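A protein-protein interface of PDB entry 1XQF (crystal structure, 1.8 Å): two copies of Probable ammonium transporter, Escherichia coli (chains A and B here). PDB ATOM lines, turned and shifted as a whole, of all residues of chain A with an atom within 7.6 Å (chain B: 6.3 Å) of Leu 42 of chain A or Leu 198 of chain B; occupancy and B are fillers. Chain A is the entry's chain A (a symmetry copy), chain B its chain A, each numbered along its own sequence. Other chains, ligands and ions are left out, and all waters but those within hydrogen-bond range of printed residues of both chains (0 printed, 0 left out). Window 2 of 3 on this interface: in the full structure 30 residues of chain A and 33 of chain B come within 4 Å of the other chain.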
ATOM      1  N   GLY A  33      -3.722 -17.818 -23.254  1.00  0.00           N
ATOM      2  CA  GLY A  33      -5.076 -17.872 -22.691  1.00  0.00           C
ATOM      3  C   GLY A  33      -5.158 -18.402 -21.267  1.00  0.00           C
ATOM      4  O   GLY A  33      -5.983 -17.941 -20.480  1.00  0.00           O
ATOM      5  N   ILE A  36      -3.020 -15.432 -18.659  1.00  0.00           N
ATOM      6  CA  ILE A  36      -3.535 -14.082 -18.361  1.00  0.00           C
ATOM      7  C   ILE A  36      -4.826 -14.108 -17.543  1.00  0.00           C
ATOM      8  O   ILE A  36      -5.422 -15.167 -17.348  1.00  0.00           O
ATOM      9  CB  ILE A  36      -3.708 -13.230 -19.652  1.00  0.00           C
ATOM     10  CG1 ILE A  36      -4.894 -13.735 -20.492  1.00  0.00           C
ATOM     11  CG2 ILE A  36      -2.403 -13.219 -20.459  1.00  0.00           C
ATOM     12  CD1 ILE A  36      -5.133 -12.961 -21.772  1.00  0.00           C
ATOM     13  N   ARG A  37      -5.240 -12.936 -17.058  1.00  0.00           N
ATOM     14  CA  ARG A  37      -6.477 -12.792 -16.296  1.00  0.00           C
ATOM     15  C   ARG A  37      -7.691 -13.166 -17.155  1.00  0.00           C
ATOM     16  O   ARG A  37      -7.734 -12.854 -18.351  1.00  0.00           O
ATOM     17  CB  ARG A  37      -6.594 -11.363 -15.740  1.00  0.00           C
ATOM     18  CG  ARG A  37      -7.840 -11.098 -14.912  1.00  0.00           C
ATOM     19  CD  ARG A  37      -7.726 -11.629 -13.493  1.00  0.00           C
ATOM     20  NE  ARG A  37      -7.196 -10.622 -12.578  1.00  0.00           N
ATOM     21  CZ  ARG A  37      -7.319 -10.668 -11.254  1.00  0.00           C
ATOM     22  NH1 ARG A  37      -7.961 -11.675 -10.674  1.00  0.00           N
ATOM     23  NH2 ARG A  37      -6.802  -9.703 -10.508  1.00  0.00           N
ATOM     24  N   GLY A  38      -8.647 -13.863 -16.539  1.00  0.00           N
ATOM     25  CA  GLY A  38      -9.848 -14.370 -17.210  1.00  0.00           C
ATOM     26  C   GLY A  38     -10.688 -13.331 -17.930  1.00  0.00           C
ATOM     27  O   GLY A  38     -11.208 -13.588 -19.021  1.00  0.00           O
ATOM     28  N   LYS A  39     -10.823 -12.155 -17.319  1.00  0.00           N
ATOM     29  CA  LYS A  39     -11.556 -11.035 -17.915  1.00  0.00           C
ATOM     30  C   LYS A  39     -10.894 -10.489 -19.192  1.00  0.00           C
ATOM     31  O   LYS A  39     -11.497  -9.698 -19.913  1.00  0.00           O
ATOM     32  CB  LYS A  39     -11.741  -9.912 -16.886  1.00  0.00           C
ATOM     33  CG  LYS A  39     -10.449  -9.214 -16.471  1.00  0.00           C
ATOM     34  CD  LYS A  39     -10.734  -8.011 -15.575  1.00  0.00           C
ATOM     35  CE  LYS A  39      -9.449  -7.288 -15.207  1.00  0.00           C
ATOM     36  NZ  LYS A  39      -9.706  -6.124 -14.313  1.00  0.00           N
ATOM     37  N   ASN A  40      -9.658 -10.914 -19.460  1.00  0.00           N
ATOM     38  CA  ASN A  40      -8.907 -10.465 -20.639  1.00  0.00           C
ATOM     39  C   ASN A  40      -8.759 -11.507 -21.756  1.00  0.00           C
ATOM     40  O   ASN A  40      -8.183 -11.219 -22.815  1.00  0.00           O
ATOM     41  CB  ASN A  40      -7.523  -9.957 -20.217  1.00  0.00           C
ATOM     42  CG  ASN A  40      -7.593  -8.719 -19.322  1.00  0.00           C
ATOM     43  OD1 ASN A  40      -8.442  -7.840 -19.502  1.00  0.00           O
ATOM     44  ND2 ASN A  40      -6.683  -8.644 -18.357  1.00  0.00           N
ATOM     45  N   VAL A  41      -9.272 -12.716 -21.528  1.00  0.00           N
ATOM     46  CA  VAL A  41      -9.008 -13.843 -22.440  1.00  0.00           C
ATOM     47  C   VAL A  41      -9.664 -13.647 -23.818  1.00  0.00           C
ATOM     48  O   VAL A  41      -9.003 -13.817 -24.850  1.00  0.00           O
ATOM     49  CB  VAL A  41      -9.398 -15.211 -21.797  1.00  0.00           C
ATOM     50  CG1 VAL A  41      -9.335 -16.352 -22.818  1.00  0.00           C
ATOM     51  CG2 VAL A  41      -8.476 -15.517 -20.619  1.00  0.00           C
ATOM     52  N   LEU A  42     -10.942 -13.265 -23.819  1.00  0.00           N
ATOM     53  CA  LEU A  42     -11.707 -13.104 -25.064  1.00  0.00           C
ATOM     54  C   LEU A  42     -11.098 -12.075 -26.023  1.00  0.00           C
ATOM     55  O   LEU A  42     -10.945 -12.341 -27.223  1.00  0.00           O
ATOM     56  CB  LEU A  42     -13.182 -12.804 -24.769  1.00  0.00           C
ATOM     57  CG  LEU A  42     -13.980 -13.922 -24.081  1.00  0.00           C
ATOM     58  CD1 LEU A  42     -15.466 -13.602 -24.097  1.00  0.00           C
ATOM     59  CD2 LEU A  42     -13.727 -15.276 -24.727  1.00  0.00           C
ATOM     60  N   SER A  43     -10.716 -10.922 -25.478  1.00  0.00           N
ATOM     61  CA  SER A  43     -10.099  -9.852 -26.265  1.00  0.00           C
ATOM     62  C   SER A  43      -8.717 -10.232 -26.837  1.00  0.00           C
ATOM     63  O   SER A  43      -8.403  -9.906 -27.990  1.00  0.00           O
ATOM     64  CB  SER A  43     -10.052  -8.552 -25.440  1.00  0.00           C
ATOM     65  OG  SER A  43      -9.444  -7.504 -26.169  1.00  0.00           O
ATOM     66  N   MET A  44      -7.901 -10.936 -26.046  1.00  0.00           N
ATOM     67  CA  MET A  44      -6.611 -11.449 -26.522  1.00  0.00           C
ATOM     68  C   MET A  44      -6.774 -12.442 -27.683  1.00  0.00           C
ATOM     69  O   MET A  44      -6.036 -12.371 -28.667  1.00  0.00           O
ATOM     70  CB  MET A  44      -5.814 -12.094 -25.377  1.00  0.00           C
ATOM     71  CG  MET A  44      -4.448 -12.727 -25.775  1.00  0.00           C
ATOM     72  SD  MET A  44      -4.487 -14.427 -26.424  1.00  0.00           S
ATOM     73  CE  MET A  44      -5.217 -15.266 -25.016  1.00  0.00           C
ATOM     74  N   LEU A  45      -7.738 -13.358 -27.561  1.00  0.00           N
ATOM     75  CA  LEU A  45      -8.004 -14.349 -28.614  1.00  0.00           C
ATOM     76  C   LEU A  45      -8.434 -13.672 -29.934  1.00  0.00           C
ATOM     77  O   LEU A  45      -8.009 -14.095 -31.017  1.00  0.00           O
ATOM     78  CB  LEU A  45      -9.042 -15.388 -28.154  1.00  0.00           C
ATOM     79  CG  LEU A  45      -8.671 -16.409 -27.054  1.00  0.00           C
ATOM     80  CD1 LEU A  45      -9.856 -17.329 -26.767  1.00  0.00           C
ATOM     81  CD2 LEU A  45      -7.440 -17.252 -27.376  1.00  0.00           C
ATOM     82  N   THR A  46      -9.237 -12.615 -29.821  1.00  0.00           N
ATOM     83  CA  THR A  46      -9.660 -11.797 -30.968  1.00  0.00           C
ATOM     84  C   THR A  46      -8.473 -11.097 -31.649  1.00  0.00           C
ATOM     85  O   THR A  46      -8.331 -11.177 -32.874  1.00  0.00           O
ATOM     86  CB  THR A  46     -10.753 -10.759 -30.580  1.00  0.00           C
ATOM     87  OG1 THR A  46     -11.813 -11.404 -29.859  1.00  0.00           O
ATOM     88  CG2 THR A  46     -11.346 -10.085 -31.830  1.00  0.00           C
ATOM     89  N   GLN A  47      -7.631 -10.423 -30.859  1.00  0.00           N
ATOM     90  CA  GLN A  47      -6.392  -9.795 -31.370  1.00  0.00           C
ATOM     91  C   GLN A  47      -5.414 -10.756 -32.065  1.00  0.00           C
ATOM     92  O   GLN A  47      -4.881 -10.428 -33.131  1.00  0.00           O
ATOM     93  CB  GLN A  47      -5.665  -9.006 -30.268  1.00  0.00           C
ATOM     94  CG  GLN A  47      -6.416  -7.765 -29.791  1.00  0.00           C
ATOM     95  CD  GLN A  47      -5.528  -6.794 -29.019  1.00  0.00           C
ATOM     96  OE1 GLN A  47      -4.298  -6.886 -29.058  1.00  0.00           O
ATOM     97  NE2 GLN A  47      -6.152  -5.859 -28.319  1.00  0.00           N
ATOM     98  N   VAL A  48      -5.181 -11.937 -31.482  1.00  0.00           N
ATOM     99  CA  VAL A  48      -4.324 -12.943 -32.130  1.00  0.00           C
ATOM    100  C   VAL A  48      -4.887 -13.386 -33.483  1.00  0.00           C
ATOM    101  O   VAL A  48      -4.142 -13.519 -34.450  1.00  0.00           O
ATOM    102  CB  VAL A  48      -4.042 -14.188 -31.217  1.00  0.00           C
ATOM    103  CG1 VAL A  48      -3.321 -15.294 -31.993  1.00  0.00           C
ATOM    104  CG2 VAL A  48      -3.215 -13.775 -29.988  1.00  0.00           C
ATOM    105  N   THR A  49      -6.201 -13.605 -33.545  1.00  0.00           N
ATOM    106  CA  THR A  49      -6.855 -14.083 -34.767  1.00  0.00           C
ATOM    107  C   THR A  49      -6.838 -13.024 -35.899  1.00  0.00           C
ATOM    108  O   THR A  49      -6.512 -13.355 -37.048  1.00  0.00           O
ATOM    109  CB  THR A  49      -8.307 -14.582 -34.464  1.00  0.00           C
ATOM    110  OG1 THR A  49      -8.259 -15.623 -33.473  1.00  0.00           O
ATOM    111  CG2 THR A  49      -9.005 -15.112 -35.727  1.00  0.00           C
ATOM    112  N   GLY B  34     -19.325 -25.389 -27.731  1.00  0.00           N
ATOM    113  CA  GLY B  34     -19.229 -24.071 -27.092  1.00  0.00           C
ATOM    114  C   GLY B  34     -20.414 -23.152 -27.356  1.00  0.00           C
ATOM    115  O   GLY B  34     -20.621 -22.174 -26.627  1.00  0.00           O
ATOM    116  N   LEU B  35     -21.175 -23.454 -28.409  1.00  0.00           N
ATOM    117  CA  LEU B  35     -22.322 -22.633 -28.830  1.00  0.00           C
ATOM    118  C   LEU B  35     -23.627 -22.964 -28.112  1.00  0.00           C
ATOM    119  O   LEU B  35     -24.381 -22.060 -27.741  1.00  0.00           O
ATOM    120  CB  LEU B  35     -22.554 -22.757 -30.340  1.00  0.00           C
ATOM    121  CG  LEU B  35     -21.604 -22.073 -31.322  1.00  0.00           C
ATOM    122  CD1 LEU B  35     -21.928 -22.524 -32.737  1.00  0.00           C
ATOM    123  CD2 LEU B  35     -21.691 -20.550 -31.204  1.00  0.00           C
ATOM    124  N   PRO B 195     -23.672 -18.194 -26.351  1.00  0.00           N
ATOM    125  CA  PRO B 195     -22.545 -19.116 -26.362  1.00  0.00           C
ATOM    126  C   PRO B 195     -21.873 -19.196 -24.992  1.00  0.00           C
ATOM    127  O   PRO B 195     -21.252 -18.225 -24.544  1.00  0.00           O
ATOM    128  CB  PRO B 195     -21.608 -18.491 -27.396  1.00  0.00           C
ATOM    129  CG  PRO B 195     -22.535 -17.770 -28.358  1.00  0.00           C
ATOM    130  CD  PRO B 195     -23.857 -17.537 -27.656  1.00  0.00           C
ATOM    131  N   HIS B 196     -21.996 -20.350 -24.338  1.00  0.00           N
ATOM    132  CA  HIS B 196     -21.552 -20.496 -22.950  1.00  0.00           C
ATOM    133  C   HIS B 196     -20.037 -20.695 -22.777  1.00  0.00           C
ATOM    134  O   HIS B 196     -19.512 -20.537 -21.668  1.00  0.00           O
ATOM    135  CB  HIS B 196     -22.341 -21.606 -22.238  1.00  0.00           C
ATOM    136  CG  HIS B 196     -21.820 -22.986 -22.497  1.00  0.00           C
ATOM    137  ND1 HIS B 196     -22.096 -23.683 -23.653  1.00  0.00           N
ATOM    138  CD2 HIS B 196     -21.043 -23.800 -21.743  1.00  0.00           C
ATOM    139  CE1 HIS B 196     -21.509 -24.866 -23.601  1.00  0.00           C
ATOM    140  NE2 HIS B 196     -20.862 -24.962 -22.454  1.00  0.00           N
ATOM    141  N   ASN B 197     -19.340 -21.036 -23.863  1.00  0.00           N
ATOM    142  CA  ASN B 197     -17.910 -21.322 -23.793  1.00  0.00           C
ATOM    143  C   ASN B 197     -17.178 -20.925 -25.081  1.00  0.00           C
ATOM    144  O   ASN B 197     -16.903 -21.774 -25.924  1.00  0.00           O
ATOM    145  CB  ASN B 197     -17.704 -22.812 -23.485  1.00  0.00           C
ATOM    146  CG  ASN B 197     -16.303 -23.133 -23.006  1.00  0.00           C
ATOM    147  OD1 ASN B 197     -15.327 -22.468 -23.361  1.00  0.00           O
ATOM    148  ND2 ASN B 197     -16.194 -24.184 -22.206  1.00  0.00           N
ATOM    149  N   LEU B 198     -16.872 -19.637 -25.226  1.00  0.00           N
ATOM    150  CA  LEU B 198     -16.206 -19.128 -26.436  1.00  0.00           C
ATOM    151  C   LEU B 198     -14.763 -19.643 -26.674  1.00  0.00           C
ATOM    152  O   LEU B 198     -14.384 -19.857 -27.828  1.00  0.00           O
ATOM    153  CB  LEU B 198     -16.289 -17.592 -26.520  1.00  0.00           C
ATOM    154  CG  LEU B 198     -17.671 -16.990 -26.838  1.00  0.00           C
ATOM    155  CD1 LEU B 198     -17.751 -15.525 -26.437  1.00  0.00           C
ATOM    156  CD2 LEU B 198     -18.039 -17.167 -28.319  1.00  0.00           C
ATOM    157  N   PRO B 199     -13.950 -19.833 -25.605  1.00  0.00           N
ATOM    158  CA  PRO B 199     -12.662 -20.521 -25.841  1.00  0.00           C
ATOM    159  C   PRO B 199     -12.782 -21.917 -26.476  1.00  0.00           C
ATOM    160  O   PRO B 199     -11.917 -22.291 -27.283  1.00  0.00           O
ATOM    161  CB  PRO B 199     -12.044 -20.603 -24.442  1.00  0.00           C
ATOM    162  CG  PRO B 199     -12.632 -19.446 -23.715  1.00  0.00           C
ATOM    163  CD  PRO B 199     -14.068 -19.404 -24.196  1.00  0.00           C
ATOM    164  N   MET B 200     -13.831 -22.667 -26.128  1.00  0.00           N
ATOM    165  CA  MET B 200     -14.137 -23.942 -26.808  1.00  0.00           C
ATOM    166  C   MET B 200     -14.525 -23.764 -28.296  1.00  0.00           C
ATOM    167  O   MET B 200     -14.096 -24.553 -29.150  1.00  0.00           O
ATOM    168  CB  MET B 200     -15.223 -24.734 -26.047  1.00  0.00           C
ATOM    169  CG  MET B 200     -15.522 -26.144 -26.613  1.00  0.00           C
ATOM    170  SD  MET B 200     -16.802 -27.064 -25.699  1.00  0.00           S
ATOM    171  CE  MET B 200     -15.912 -27.503 -24.207  1.00  0.00           C
ATOM    172  N   VAL B 201     -15.345 -22.750 -28.598  1.00  0.00           N
ATOM    173  CA  VAL B 201     -15.693 -22.415 -29.991  1.00  0.00           C
ATOM    174  C   VAL B 201     -14.430 -22.064 -30.801  1.00  0.00           C
ATOM    175  O   VAL B 201     -14.265 -22.529 -31.940  1.00  0.00           O
ATOM    176  CB  VAL B 201     -16.732 -21.238 -30.089  1.00  0.00           C
ATOM    177  CG1 VAL B 201     -16.974 -20.820 -31.546  1.00  0.00           C
ATOM    178  CG2 VAL B 201     -18.056 -21.603 -29.424  1.00  0.00           C
ATOM    179  N   PHE B 202     -13.545 -21.254 -30.214  1.00  0.00           N
ATOM    180  CA  PHE B 202     -12.275 -20.890 -30.881  1.00  0.00           C
ATOM    181  C   PHE B 202     -11.407 -22.137 -31.165  1.00  0.00           C
ATOM    182  O   PHE B 202     -10.822 -22.276 -32.244  1.00  0.00           O
ATOM    183  CB  PHE B 202     -11.480 -19.861 -30.039  1.00  0.00           C
ATOM    184  CG  PHE B 202     -10.057 -19.650 -30.526  1.00  0.00           C
ATOM    185  CD1 PHE B 202      -9.787 -18.794 -31.602  1.00  0.00           C
ATOM    186  CD2 PHE B 202      -8.994 -20.325 -29.922  1.00  0.00           C
ATOM    187  CE1 PHE B 202      -8.484 -18.607 -32.066  1.00  0.00           C
ATOM    188  CE2 PHE B 202      -7.686 -20.154 -30.381  1.00  0.00           C
ATOM    189  CZ  PHE B 202      -7.434 -19.292 -31.455  1.00  0.00           C
ATOM    190  N   THR B 203     -11.327 -23.038 -30.191  1.00  0.00           N
ATOM    191  CA  THR B 203     -10.534 -24.276 -30.341  1.00  0.00           C
ATOM    192  C   THR B 203     -11.070 -25.158 -31.485  1.00  0.00           C
ATOM    193  O   THR B 203     -10.295 -25.659 -32.312  1.00  0.00           O
ATOM    194  CB  THR B 203     -10.457 -25.068 -28.999  1.00  0.00           C
ATOM    195  OG1 THR B 203      -9.891 -24.241 -27.978  1.00  0.00           O
ATOM    196  CG2 THR B 203      -9.586 -26.332 -29.137  1.00  0.00           C
ATOM    197  N   LEU B 258     -15.012 -11.988 -30.798  1.00  0.00           N
ATOM    198  CA  LEU B 258     -14.399 -13.299 -31.020  1.00  0.00           C
ATOM    199  C   LEU B 258     -15.257 -14.215 -31.895  1.00  0.00           C
ATOM    200  O   LEU B 258     -14.731 -14.852 -32.813  1.00  0.00           O
ATOM    201  CB  LEU B 258     -14.015 -13.993 -29.700  1.00  0.00           C
ATOM    202  CG  LEU B 258     -13.337 -15.383 -29.823  1.00  0.00           C
ATOM    203  CD1 LEU B 258     -12.045 -15.344 -30.656  1.00  0.00           C
ATOM    204  CD2 LEU B 258     -13.063 -15.995 -28.453  1.00  0.00           C
ATOM    205  N   LEU B 259     -16.567 -14.275 -31.627  1.00  0.00           N
ATOM    206  CA  LEU B 259     -17.465 -15.099 -32.450  1.00  0.00           C
ATOM    207  C   LEU B 259     -17.506 -14.611 -33.905  1.00  0.00           C
ATOM    208  O   LEU B 259     -17.584 -15.424 -34.830  1.00  0.00           O
ATOM    209  CB  LEU B 259     -18.886 -15.174 -31.854  1.00  0.00           C
ATOM    210  CG  LEU B 259     -19.923 -16.080 -32.544  1.00  0.00           C
ATOM    211  CD1 LEU B 259     -19.420 -17.520 -32.712  1.00  0.00           C
ATOM    212  CD2 LEU B 259     -21.247 -16.056 -31.789  1.00  0.00           C
ATOM    213  N   CYS B 262     -14.201 -15.871 -35.696  1.00  0.00           N
ATOM    214  CA  CYS B 262     -14.307 -17.306 -35.993  1.00  0.00           C
ATOM    215  C   CYS B 262     -15.302 -17.561 -37.143  1.00  0.00           C
ATOM    216  O   CYS B 262     -15.039 -18.402 -38.012  1.00  0.00           O
ATOM    217  CB  CYS B 262     -14.707 -18.117 -34.741  1.00  0.00           C
ATOM    218  SG  CYS B 262     -13.524 -18.138 -33.333  1.00  0.00           S
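N of Leu 258 of chain B lies within hydrogen-bond range of OG1 of Thr 46 of chain A, at 3.4 Å.
Gly 38 of chain A touches none of the printed residues of chain B.
Leu 42 of chain A touches just these residues of chain B: Leu 198 (3.8 Å) and Leu 258 (3.9 Å).
Printed residues of chain B within 4 Å of Leu 45 of chain A: Leu 258.
Of the printed residues of chain B, Thr 46 of chain A touches Leu 258.
Of the printed residues of chain B, Thr 49 of chain A touches Phe 202 (3.3 Å).
Of chain A, only Leu 42 (3.8 Å) comes within 4 Å of Leu 198 of chain B.
Pro 199 of chain B touches none of the printed residues of chain A.
Printed residues of chain A within 4 Å of Phe 202 of chain B: Thr 49.
Printed residues of chain A within 4 Å of Leu 258 of chain B: Leu 42, Leu 45 and Thr 46.
The nearest residue of chain A that does not touch Leu 198 of chain B is Leu 45 of chain A (5.3 Å).
Among the printed residues, pairs that only touch across the chains: Leu 42 of chain A with Leu 198 of chain B (3.8 Å), Leu 42 of chain A with Leu 258 of chain B (3.9 Å), Leu 45 of chain A with Leu 258 of chain B (3.9 Å) and Thr 49 of chain A with Phe 202 of chain B (3.3 Å).
Printed residues of chain A that touch a printed residue of chain B: Leu 42, Leu 45, Thr 46 and Thr 49.
Hydrophobic or aromatic side chains of chain A that line the printed part of chain B: Leu 42 and Leu 45.
Along chain A the printed residues that touch a printed residue of chain B span positions 42 to 49.
Among the printed residues, 5 pairs touch across the chains.
No position is printed for both chains.
The backbone carbonyl oxygen (O) of Leu 258 of chain B lies within hydrogen-bond range of the side-chain sulfur (SG) of Cys 262 of chain B (3.5 Å).
The backbone carbonyl oxygen (O) of Leu 42 of chain A lies within hydrogen-bond range of the side-chain hydroxyl (OG1) of Thr 46 of chain A, at 2.9 Å.
The side-chain hydroxyl (OG1) of Thr 49 of chain A is in hydrogen-bond range of the backbone carbonyl oxygen (O) of Leu 45 of chain A (2.9 Å).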
